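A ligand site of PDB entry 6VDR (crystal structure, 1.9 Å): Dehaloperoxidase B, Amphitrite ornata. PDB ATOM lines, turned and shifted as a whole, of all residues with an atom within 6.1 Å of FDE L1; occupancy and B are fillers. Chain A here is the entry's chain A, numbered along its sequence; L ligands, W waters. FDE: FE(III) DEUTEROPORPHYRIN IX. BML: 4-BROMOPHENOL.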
ATOM      1  N   PHE A  21      -3.767   1.311  -6.149  1.00  0.00           N
ATOM      2  CA  PHE A  21      -3.378   0.079  -6.861  1.00  0.00           C
ATOM      3  C   PHE A  21      -2.587  -0.843  -5.907  1.00  0.00           C
ATOM      4  O   PHE A  21      -2.834  -2.060  -5.902  1.00  0.00           O
ATOM      5  CB  PHE A  21      -2.642   0.430  -8.153  1.00  0.00           C
ATOM      6  CG  PHE A  21      -2.738  -0.674  -9.160  1.00  0.00           C
ATOM      7  CD1 PHE A  21      -3.941  -0.886  -9.826  1.00  0.00           C
ATOM      8  CD2 PHE A  21      -1.691  -1.542  -9.368  1.00  0.00           C
ATOM      9  CE1 PHE A  21      -4.067  -1.938 -10.719  1.00  0.00           C
ATOM     10  CE2 PHE A  21      -1.820  -2.581 -10.259  1.00  0.00           C
ATOM     11  CZ  PHE A  21      -3.008  -2.779 -10.934  1.00  0.00           C
ATOM     12  N   ARG A  33      -0.102 -11.822 -10.205  1.00  0.00           N
ATOM     13  CA  ARG A  33       0.104 -12.830 -11.275  1.00  0.00           C
ATOM     14  C   ARG A  33      -0.163 -12.237 -12.661  1.00  0.00           C
ATOM     15  O   ARG A  33       0.451 -12.725 -13.613  1.00  0.00           O
ATOM     16  CB  ARG A  33      -0.835 -14.013 -11.088  1.00  0.00           C
ATOM     17  CG  ARG A  33      -0.250 -15.104 -10.204  1.00  0.00           C
ATOM     18  CD  ARG A  33      -0.564 -14.935  -8.732  1.00  0.00           C
ATOM     19  NE  ARG A  33      -1.213 -16.112  -8.160  1.00  0.00           N
ATOM     20  CZ  ARG A  33      -2.400 -16.600  -8.539  1.00  0.00           C
ATOM     21  NH1 ARG A  33      -3.071 -16.059  -9.547  1.00  0.00           N
ATOM     22  NH2 ARG A  33      -2.912 -17.641  -7.914  1.00  0.00           N
ATOM     23  N   ASN A  34      -1.073 -11.278 -12.790  1.00  0.00           N
ATOM     24  CA  ASN A  34      -1.479 -10.760 -14.122  1.00  0.00           C
ATOM     25  C   ASN A  34      -0.443  -9.751 -14.620  1.00  0.00           C
ATOM     26  O   ASN A  34      -0.583  -9.341 -15.790  1.00  0.00           O
ATOM     27  CB  ASN A  34      -2.892 -10.183 -14.107  1.00  0.00           C
ATOM     28  CG  ASN A  34      -3.938 -11.256 -13.875  1.00  0.00           C
ATOM     29  OD1 ASN A  34      -3.898 -12.299 -14.518  1.00  0.00           O
ATOM     30  ND2 ASN A  34      -4.824 -11.038 -12.927  1.00  0.00           N
ATOM     31  N   PHE A  35       0.536  -9.366 -13.799  1.00  0.00           N
ATOM     32  CA  PHE A  35       1.508  -8.271 -14.102  1.00  0.00           C
ATOM     33  C   PHE A  35       2.940  -8.826 -14.046  1.00  0.00           C
ATOM     34  O   PHE A  35       3.359  -9.340 -12.984  1.00  0.00           O
ATOM     35  CB  PHE A  35       1.318  -7.105 -13.125  1.00  0.00           C
ATOM     36  CG  PHE A  35      -0.034  -6.445 -13.209  1.00  0.00           C
ATOM     37  CD1 PHE A  35      -0.285  -5.472 -14.165  1.00  0.00           C
ATOM     38  CD2 PHE A  35      -1.075  -6.850 -12.387  1.00  0.00           C
ATOM     39  CE1 PHE A  35      -1.538  -4.899 -14.264  1.00  0.00           C
ATOM     40  CE2 PHE A  35      -2.323  -6.255 -12.477  1.00  0.00           C
ATOM     41  CZ  PHE A  35      -2.552  -5.277 -13.424  1.00  0.00           C
ATOM     42  N   LYS A  36       3.665  -8.750 -15.176  1.00  0.00           N
ATOM     43  CA  LYS A  36       5.043  -9.304 -15.287  1.00  0.00           C
ATOM     44  C   LYS A  36       5.932  -8.647 -14.230  1.00  0.00           C
ATOM     45  O   LYS A  36       5.996  -7.407 -14.212  1.00  0.00           O
ATOM     46  CB  LYS A  36       5.602  -9.125 -16.703  1.00  0.00           C
ATOM     47  CG  LYS A  36       4.981 -10.024 -17.766  1.00  0.00           C
ATOM     48  CD  LYS A  36       4.340 -11.303 -17.235  1.00  0.00           C
ATOM     49  CE  LYS A  36       3.685 -12.166 -18.300  1.00  0.00           C
ATOM     50  NZ  LYS A  36       2.545 -12.932 -17.747  1.00  0.00           N
ATOM     51  N   ASN A  37       6.500  -9.452 -13.335  1.00  0.00           N
ATOM     52  CA  ASN A  37       7.583  -9.080 -12.402  1.00  0.00           C
ATOM     53  C   ASN A  37       7.035  -8.349 -11.172  1.00  0.00           C
ATOM     54  O   ASN A  37       7.849  -7.755 -10.483  1.00  0.00           O
ATOM     55  CB  ASN A  37       8.646  -8.189 -13.061  1.00  0.00           C
ATOM     56  CG  ASN A  37       9.526  -8.944 -14.040  1.00  0.00           C
ATOM     57  OD1 ASN A  37       9.326 -10.139 -14.268  1.00  0.00           O
ATOM     58  ND2 ASN A  37      10.476  -8.244 -14.626  1.00  0.00           N
ATOM     59  N   LYS A  51       7.439   0.749 -15.414  1.00  0.00           N
ATOM     60  CA  LYS A  51       6.142   0.325 -16.020  1.00  0.00           C
ATOM     61  C   LYS A  51       5.044   0.291 -14.959  1.00  0.00           C
ATOM     62  O   LYS A  51       3.886   0.516 -15.321  1.00  0.00           O
ATOM     63  CB  LYS A  51       6.265  -1.038 -16.704  1.00  0.00           C
ATOM     64  CG  LYS A  51       6.823  -0.958 -18.119  1.00  0.00           C
ATOM     65  CD  LYS A  51       6.693  -2.243 -18.938  1.00  0.00           C
ATOM     66  CE  LYS A  51       6.919  -1.958 -20.413  1.00  0.00           C
ATOM     67  NZ  LYS A  51       7.439  -3.139 -21.150  1.00  0.00           N
ATOM     68  N   HIS A  55       2.106   2.325 -16.117  1.00  0.00           N
ATOM     69  CA  HIS A  55       0.882   1.523 -16.401  1.00  0.00           C
ATOM     70  C   HIS A  55      -0.219   1.866 -15.386  1.00  0.00           C
ATOM     71  O   HIS A  55      -1.368   2.100 -15.825  1.00  0.00           O
ATOM     72  CB  HIS A  55       1.160   0.026 -16.460  1.00  0.00           C
ATOM     73  CG  HIS A  55      -0.068  -0.735 -16.848  1.00  0.00           C
ATOM     74  ND1 HIS A  55      -0.885  -1.298 -15.908  1.00  0.00           N
ATOM     75  CD2 HIS A  55      -0.673  -0.921 -18.040  1.00  0.00           C
ATOM     76  CE1 HIS A  55      -1.891  -1.901 -16.498  1.00  0.00           C
ATOM     77  NE2 HIS A  55      -1.801  -1.665 -17.815  1.00  0.00           N
ATOM     78  N   LYS A  58      -1.876   5.074 -16.189  1.00  0.00           N
ATOM     79  CA  LYS A  58      -2.686   4.944 -17.440  1.00  0.00           C
ATOM     80  C   LYS A  58      -4.011   4.240 -17.149  1.00  0.00           C
ATOM     81  O   LYS A  58      -5.058   4.687 -17.677  1.00  0.00           O
ATOM     82  CB  LYS A  58      -1.868   4.270 -18.546  1.00  0.00           C
ATOM     83  CG  LYS A  58      -0.821   5.182 -19.147  1.00  0.00           C
ATOM     84  CD  LYS A  58       0.000   4.548 -20.220  1.00  0.00           C
ATOM     85  CE  LYS A  58       0.925   5.548 -20.884  1.00  0.00           C
ATOM     86  NZ  LYS A  58       2.270   4.990 -21.105  1.00  0.00           N
ATOM     87  N   VAL A  59      -3.990   3.228 -16.271  1.00  0.00           N
ATOM     88  CA  VAL A  59      -5.230   2.555 -15.772  1.00  0.00           C
ATOM     89  C   VAL A  59      -6.143   3.599 -15.139  1.00  0.00           C
ATOM     90  O   VAL A  59      -7.339   3.662 -15.501  1.00  0.00           O
ATOM     91  CB  VAL A  59      -4.888   1.422 -14.779  1.00  0.00           C
ATOM     92  CG1 VAL A  59      -6.138   0.894 -14.073  1.00  0.00           C
ATOM     93  CG2 VAL A  59      -4.137   0.291 -15.486  1.00  0.00           C
ATOM     94  N   LEU A  62      -7.613   6.270 -17.536  1.00  0.00           N
ATOM     95  CA  LEU A  62      -8.751   5.690 -18.291  1.00  0.00           C
ATOM     96  C   LEU A  62      -9.973   5.616 -17.365  1.00  0.00           C
ATOM     97  O   LEU A  62     -11.048   6.048 -17.780  1.00  0.00           O
ATOM     98  CB  LEU A  62      -8.379   4.317 -18.885  1.00  0.00           C
ATOM     99  CG  LEU A  62      -9.427   3.623 -19.769  1.00  0.00           C
ATOM    100  CD1 LEU A  62     -10.046   4.594 -20.786  1.00  0.00           C
ATOM    101  CD2 LEU A  62      -8.821   2.440 -20.514  1.00  0.00           C
ATOM    102  N   MET A  63      -9.827   5.108 -16.139  1.00  0.00           N
ATOM    103  CA  MET A  63     -10.993   5.053 -15.225  1.00  0.00           C
ATOM    104  C   MET A  63     -11.523   6.471 -14.957  1.00  0.00           C
ATOM    105  O   MET A  63     -12.734   6.626 -14.893  1.00  0.00           O
ATOM    106  CB  MET A  63     -10.711   4.300 -13.921  1.00  0.00           C
ATOM    107  CG  MET A  63     -11.699   3.134 -13.703  1.00  0.00           C
ATOM    108  SD  MET A  63     -11.193   1.569 -14.454  1.00  0.00           S
ATOM    109  CE  MET A  63     -11.471   1.852 -16.201  1.00  0.00           C
ATOM    110  N   LEU A  83     -13.405  -0.540 -23.988  1.00  0.00           N
ATOM    111  CA  LEU A  83     -12.553  -1.176 -22.942  1.00  0.00           C
ATOM    112  C   LEU A  83     -12.391  -2.668 -23.248  1.00  0.00           C
ATOM    113  O   LEU A  83     -11.254  -3.165 -23.252  1.00  0.00           O
ATOM    114  CB  LEU A  83     -13.196  -0.967 -21.567  1.00  0.00           C
ATOM    115  CG  LEU A  83     -12.618   0.152 -20.703  1.00  0.00           C
ATOM    116  CD1 LEU A  83     -13.583   0.514 -19.574  1.00  0.00           C
ATOM    117  CD2 LEU A  83     -11.267  -0.259 -20.120  1.00  0.00           C
ATOM    118  N   MET A  86     -10.042  -3.179 -26.227  1.00  0.00           N
ATOM    119  CA  MET A  86      -8.678  -2.578 -26.164  1.00  0.00           C
ATOM    120  C   MET A  86      -7.642  -3.613 -26.613  1.00  0.00           C
ATOM    121  O   MET A  86      -7.691  -4.769 -26.107  1.00  0.00           O
ATOM    122  CB  MET A  86      -8.304  -2.144 -24.752  1.00  0.00           C
ATOM    123  CG  MET A  86      -8.573  -0.694 -24.473  1.00  0.00           C
ATOM    124  SD  MET A  86      -8.233  -0.355 -22.743  1.00  0.00           S
ATOM    125  CE  MET A  86      -6.464  -0.635 -22.690  1.00  0.00           C
ATOM    126  N   GLN A  88      -4.308  -5.722 -26.779  1.00  0.00           N
ATOM    127  CA  GLN A  88      -3.727  -6.339 -25.559  1.00  0.00           C
ATOM    128  C   GLN A  88      -4.871  -6.224 -24.553  1.00  0.00           C
ATOM    129  O   GLN A  88      -5.874  -5.612 -24.931  1.00  0.00           O
ATOM    130  CB  GLN A  88      -2.393  -5.637 -25.239  1.00  0.00           C
ATOM    131  CG  GLN A  88      -1.594  -5.303 -26.500  1.00  0.00           C
ATOM    132  CD  GLN A  88      -0.270  -4.596 -26.304  1.00  0.00           C
ATOM    133  OE1 GLN A  88      -0.102  -3.430 -26.673  1.00  0.00           O
ATOM    134  NE2 GLN A  88       0.689  -5.296 -25.731  1.00  0.00           N
ATOM    135  N   HIS A  89      -4.832  -6.832 -23.366  1.00  0.00           N
ATOM    136  CA  HIS A  89      -5.956  -6.713 -22.395  1.00  0.00           C
ATOM    137  C   HIS A  89      -7.132  -7.621 -22.758  1.00  0.00           C
ATOM    138  O   HIS A  89      -8.228  -7.401 -22.221  1.00  0.00           O
ATOM    139  CB  HIS A  89      -6.480  -5.260 -22.333  1.00  0.00           C
ATOM    140  CG  HIS A  89      -5.418  -4.278 -22.028  1.00  0.00           C
ATOM    141  ND1 HIS A  89      -4.713  -3.604 -23.015  1.00  0.00           N
ATOM    142  CD2 HIS A  89      -4.885  -3.879 -20.850  1.00  0.00           C
ATOM    143  CE1 HIS A  89      -3.811  -2.825 -22.454  1.00  0.00           C
ATOM    144  NE2 HIS A  89      -3.906  -2.981 -21.134  1.00  0.00           N
ATOM    145  N   LEU A  92      -8.539  -9.460 -19.550  1.00  0.00           N
ATOM    146  CA  LEU A  92      -9.236  -8.717 -18.461  1.00  0.00           C
ATOM    147  C   LEU A  92     -10.542  -9.448 -18.075  1.00  0.00           C
ATOM    148  O   LEU A  92     -11.243  -9.920 -18.980  1.00  0.00           O
ATOM    149  CB  LEU A  92      -9.488  -7.267 -18.894  1.00  0.00           C
ATOM    150  CG  LEU A  92      -8.548  -6.201 -18.321  1.00  0.00           C
ATOM    151  CD1 LEU A  92      -7.128  -6.713 -18.116  1.00  0.00           C
ATOM    152  CD2 LEU A  92      -8.550  -4.942 -19.200  1.00  0.00           C
ATOM    153  N   PHE A  97     -11.947  -6.373 -11.687  1.00  0.00           N
ATOM    154  CA  PHE A  97     -12.506  -5.003 -11.566  1.00  0.00           C
ATOM    155  C   PHE A  97     -13.369  -4.944 -10.300  1.00  0.00           C
ATOM    156  O   PHE A  97     -13.220  -3.948  -9.588  1.00  0.00           O
ATOM    157  CB  PHE A  97     -13.201  -4.558 -12.855  1.00  0.00           C
ATOM    158  CG  PHE A  97     -12.267  -4.165 -13.977  1.00  0.00           C
ATOM    159  CD1 PHE A  97     -11.577  -2.971 -13.945  1.00  0.00           C
ATOM    160  CD2 PHE A  97     -12.099  -4.990 -15.083  1.00  0.00           C
ATOM    161  CE1 PHE A  97     -10.729  -2.612 -14.988  1.00  0.00           C
ATOM    162  CE2 PHE A  97     -11.255  -4.640 -16.123  1.00  0.00           C
ATOM    163  CZ  PHE A  97     -10.580  -3.438 -16.081  1.00  0.00           C
ATOM    164  N   LEU A 100     -10.683  -4.366  -7.663  1.00  0.00           N
ATOM    165  CA  LEU A 100     -10.056  -3.024  -7.757  1.00  0.00           C
ATOM    166  C   LEU A 100     -10.951  -1.989  -7.088  1.00  0.00           C
ATOM    167  O   LEU A 100     -10.427  -1.133  -6.343  1.00  0.00           O
ATOM    168  CB  LEU A 100      -9.845  -2.667  -9.235  1.00  0.00           C
ATOM    169  CG  LEU A 100      -9.322  -1.246  -9.440  1.00  0.00           C
ATOM    170  CD1 LEU A 100      -7.990  -1.060  -8.714  1.00  0.00           C
ATOM    171  CD2 LEU A 100      -9.222  -0.958 -10.929  1.00  0.00           C
HETATM  172  CHA FDE L   1      -0.760  -4.919 -20.145  1.00  0.00           C
HETATM  173  C1A FDE L   1      -0.506  -3.663 -20.807  1.00  0.00           C
HETATM  174  C2A FDE L   1       0.568  -3.452 -21.817  1.00  0.00           C
HETATM  175  CAA FDE L   1       1.649  -4.469 -22.212  1.00  0.00           C
HETATM  176  CBA FDE L   1       3.031  -3.933 -22.636  1.00  0.00           C
HETATM  177  CGA FDE L   1       3.679  -3.011 -21.614  1.00  0.00           C
HETATM  178  O1A FDE L   1       4.077  -3.464 -20.515  1.00  0.00           O
HETATM  179  O2A FDE L   1       3.826  -1.811 -21.923  1.00  0.00           O
HETATM  180  C3A FDE L   1       0.374  -2.068 -22.287  1.00  0.00           C
HETATM  181  CMA FDE L   1       1.220  -1.245 -23.245  1.00  0.00           C
HETATM  182  C4A FDE L   1      -0.778  -1.553 -21.501  1.00  0.00           C
HETATM  183  NA  FDE L   1      -1.449  -2.581 -20.725  1.00  0.00           N
HETATM  184  CHB FDE L   1      -1.339  -0.219 -21.700  1.00  0.00           C
HETATM  185  C1B FDE L   1      -2.570   0.256 -21.065  1.00  0.00           C
HETATM  186  C2B FDE L   1      -3.033   1.504 -21.445  1.00  0.00           C
HETATM  187  C3B FDE L   1      -4.202   1.607 -20.696  1.00  0.00           C
HETATM  188  CME FDE L   1      -5.032   2.863 -20.794  1.00  0.00           C
HETATM  189  C4B FDE L   1      -4.338   0.352 -19.931  1.00  0.00           C
HETATM  190  NB  FDE L   1      -3.293  -0.435 -20.173  1.00  0.00           N
HETATM  191  CHC FDE L   1      -5.463   0.034 -19.031  1.00  0.00           C
HETATM  192  C1C FDE L   1      -5.563  -1.207 -18.242  1.00  0.00           C
HETATM  193  C2C FDE L   1      -6.600  -1.371 -17.339  1.00  0.00           C
HETATM  194  C3C FDE L   1      -6.309  -2.576 -16.753  1.00  0.00           C
HETATM  195  CMF FDE L   1      -7.200  -3.124 -15.695  1.00  0.00           C
HETATM  196  C4C FDE L   1      -5.090  -3.038 -17.357  1.00  0.00           C
HETATM  197  NC  FDE L   1      -4.647  -2.165 -18.271  1.00  0.00           N
HETATM  198  CHD FDE L   1      -4.481  -4.296 -17.046  1.00  0.00           C
HETATM  199  C1D FDE L   1      -3.359  -4.875 -17.741  1.00  0.00           C
HETATM  200  C2D FDE L   1      -2.906  -6.239 -17.438  1.00  0.00           C
HETATM  201  CMD FDE L   1      -3.434  -7.213 -16.445  1.00  0.00           C
HETATM  202  C3D FDE L   1      -1.802  -6.422 -18.383  1.00  0.00           C
HETATM  203  CAD FDE L   1      -0.871  -7.596 -18.588  1.00  0.00           C
HETATM  204  CBD FDE L   1       0.492  -7.233 -17.989  1.00  0.00           C
HETATM  205  CGD FDE L   1       1.528  -8.270 -18.356  1.00  0.00           C
HETATM  206  O1D FDE L   1       2.118  -8.865 -17.427  1.00  0.00           O
HETATM  207  O2D FDE L   1       1.752  -8.484 -19.580  1.00  0.00           O
HETATM  208  C4D FDE L   1      -1.758  -5.151 -19.101  1.00  0.00           C
HETATM  209  ND  FDE L   1      -2.685  -4.265 -18.720  1.00  0.00           N
HETATM  210 FE   FDE L   1      -2.961  -2.347 -19.435  1.00  0.00          FE
HETATM  211  O1  BML L   2      -8.318  -8.976 -15.059  1.00  0.00           O
HETATM  212  C1  BML L   2      -7.986  -7.787 -14.476  1.00  0.00           C
HETATM  213  C2  BML L   2      -8.910  -6.753 -14.466  1.00  0.00           C
HETATM  214  C3  BML L   2      -8.590  -5.546 -13.876  1.00  0.00           C
HETATM  215  C4  BML L   2      -7.349  -5.382 -13.294  1.00  0.00           C
HETATM  216  C5  BML L   2      -6.412  -6.398 -13.300  1.00  0.00           C
HETATM  217  C6  BML L   2      -6.736  -7.614 -13.888  1.00  0.00           C
HETATM  218 BR4  BML L   2      -6.925  -3.711 -12.497  1.00  0.00          BR
HETATM  219  O   HOH W   1      -5.013   6.174 -20.058  1.00  0.00           O
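An oxygen (O1D) of FDE L1 lies close to the backbone carbonyl oxygen of Asn 34, 3.2 Å away. Merely in contact with FDE L1: Phe 97, Phe 35, Val 59, Lys 58, Met 86, Gln 88, Leu 92 and Leu 62. Hydrophobic or aromatic side chains that line FDE L1: Phe 35, His 55, Val 59, Leu 62, Met 86, His 89, Leu 92 and Phe 97. Within 4 Å of FDE L1: Asn 34, Phe 35, Lys 36, Lys 51, His 55, Lys 58, Val 59, Leu 62, Met 86, Gln 88, His 89, Leu 92 and Phe 97. Along chain A the residues within 4 Å of FDE L1 span positions 34 to 97.
A ring nitrogen (NE2) of His 89 binds an iron atom (FE) of FDE L1. A ring nitrogen (NE2) of His 55 is bound to an iron atom (FE) of FDE L1 (2.1 Å). N of Lys 36 is in hydrogen-bond range of O1D of FDE L1 (2.7 Å). NZ of Lys 51 lies within salt-bridge range of O1A of FDE L1, 3.4 Å away.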
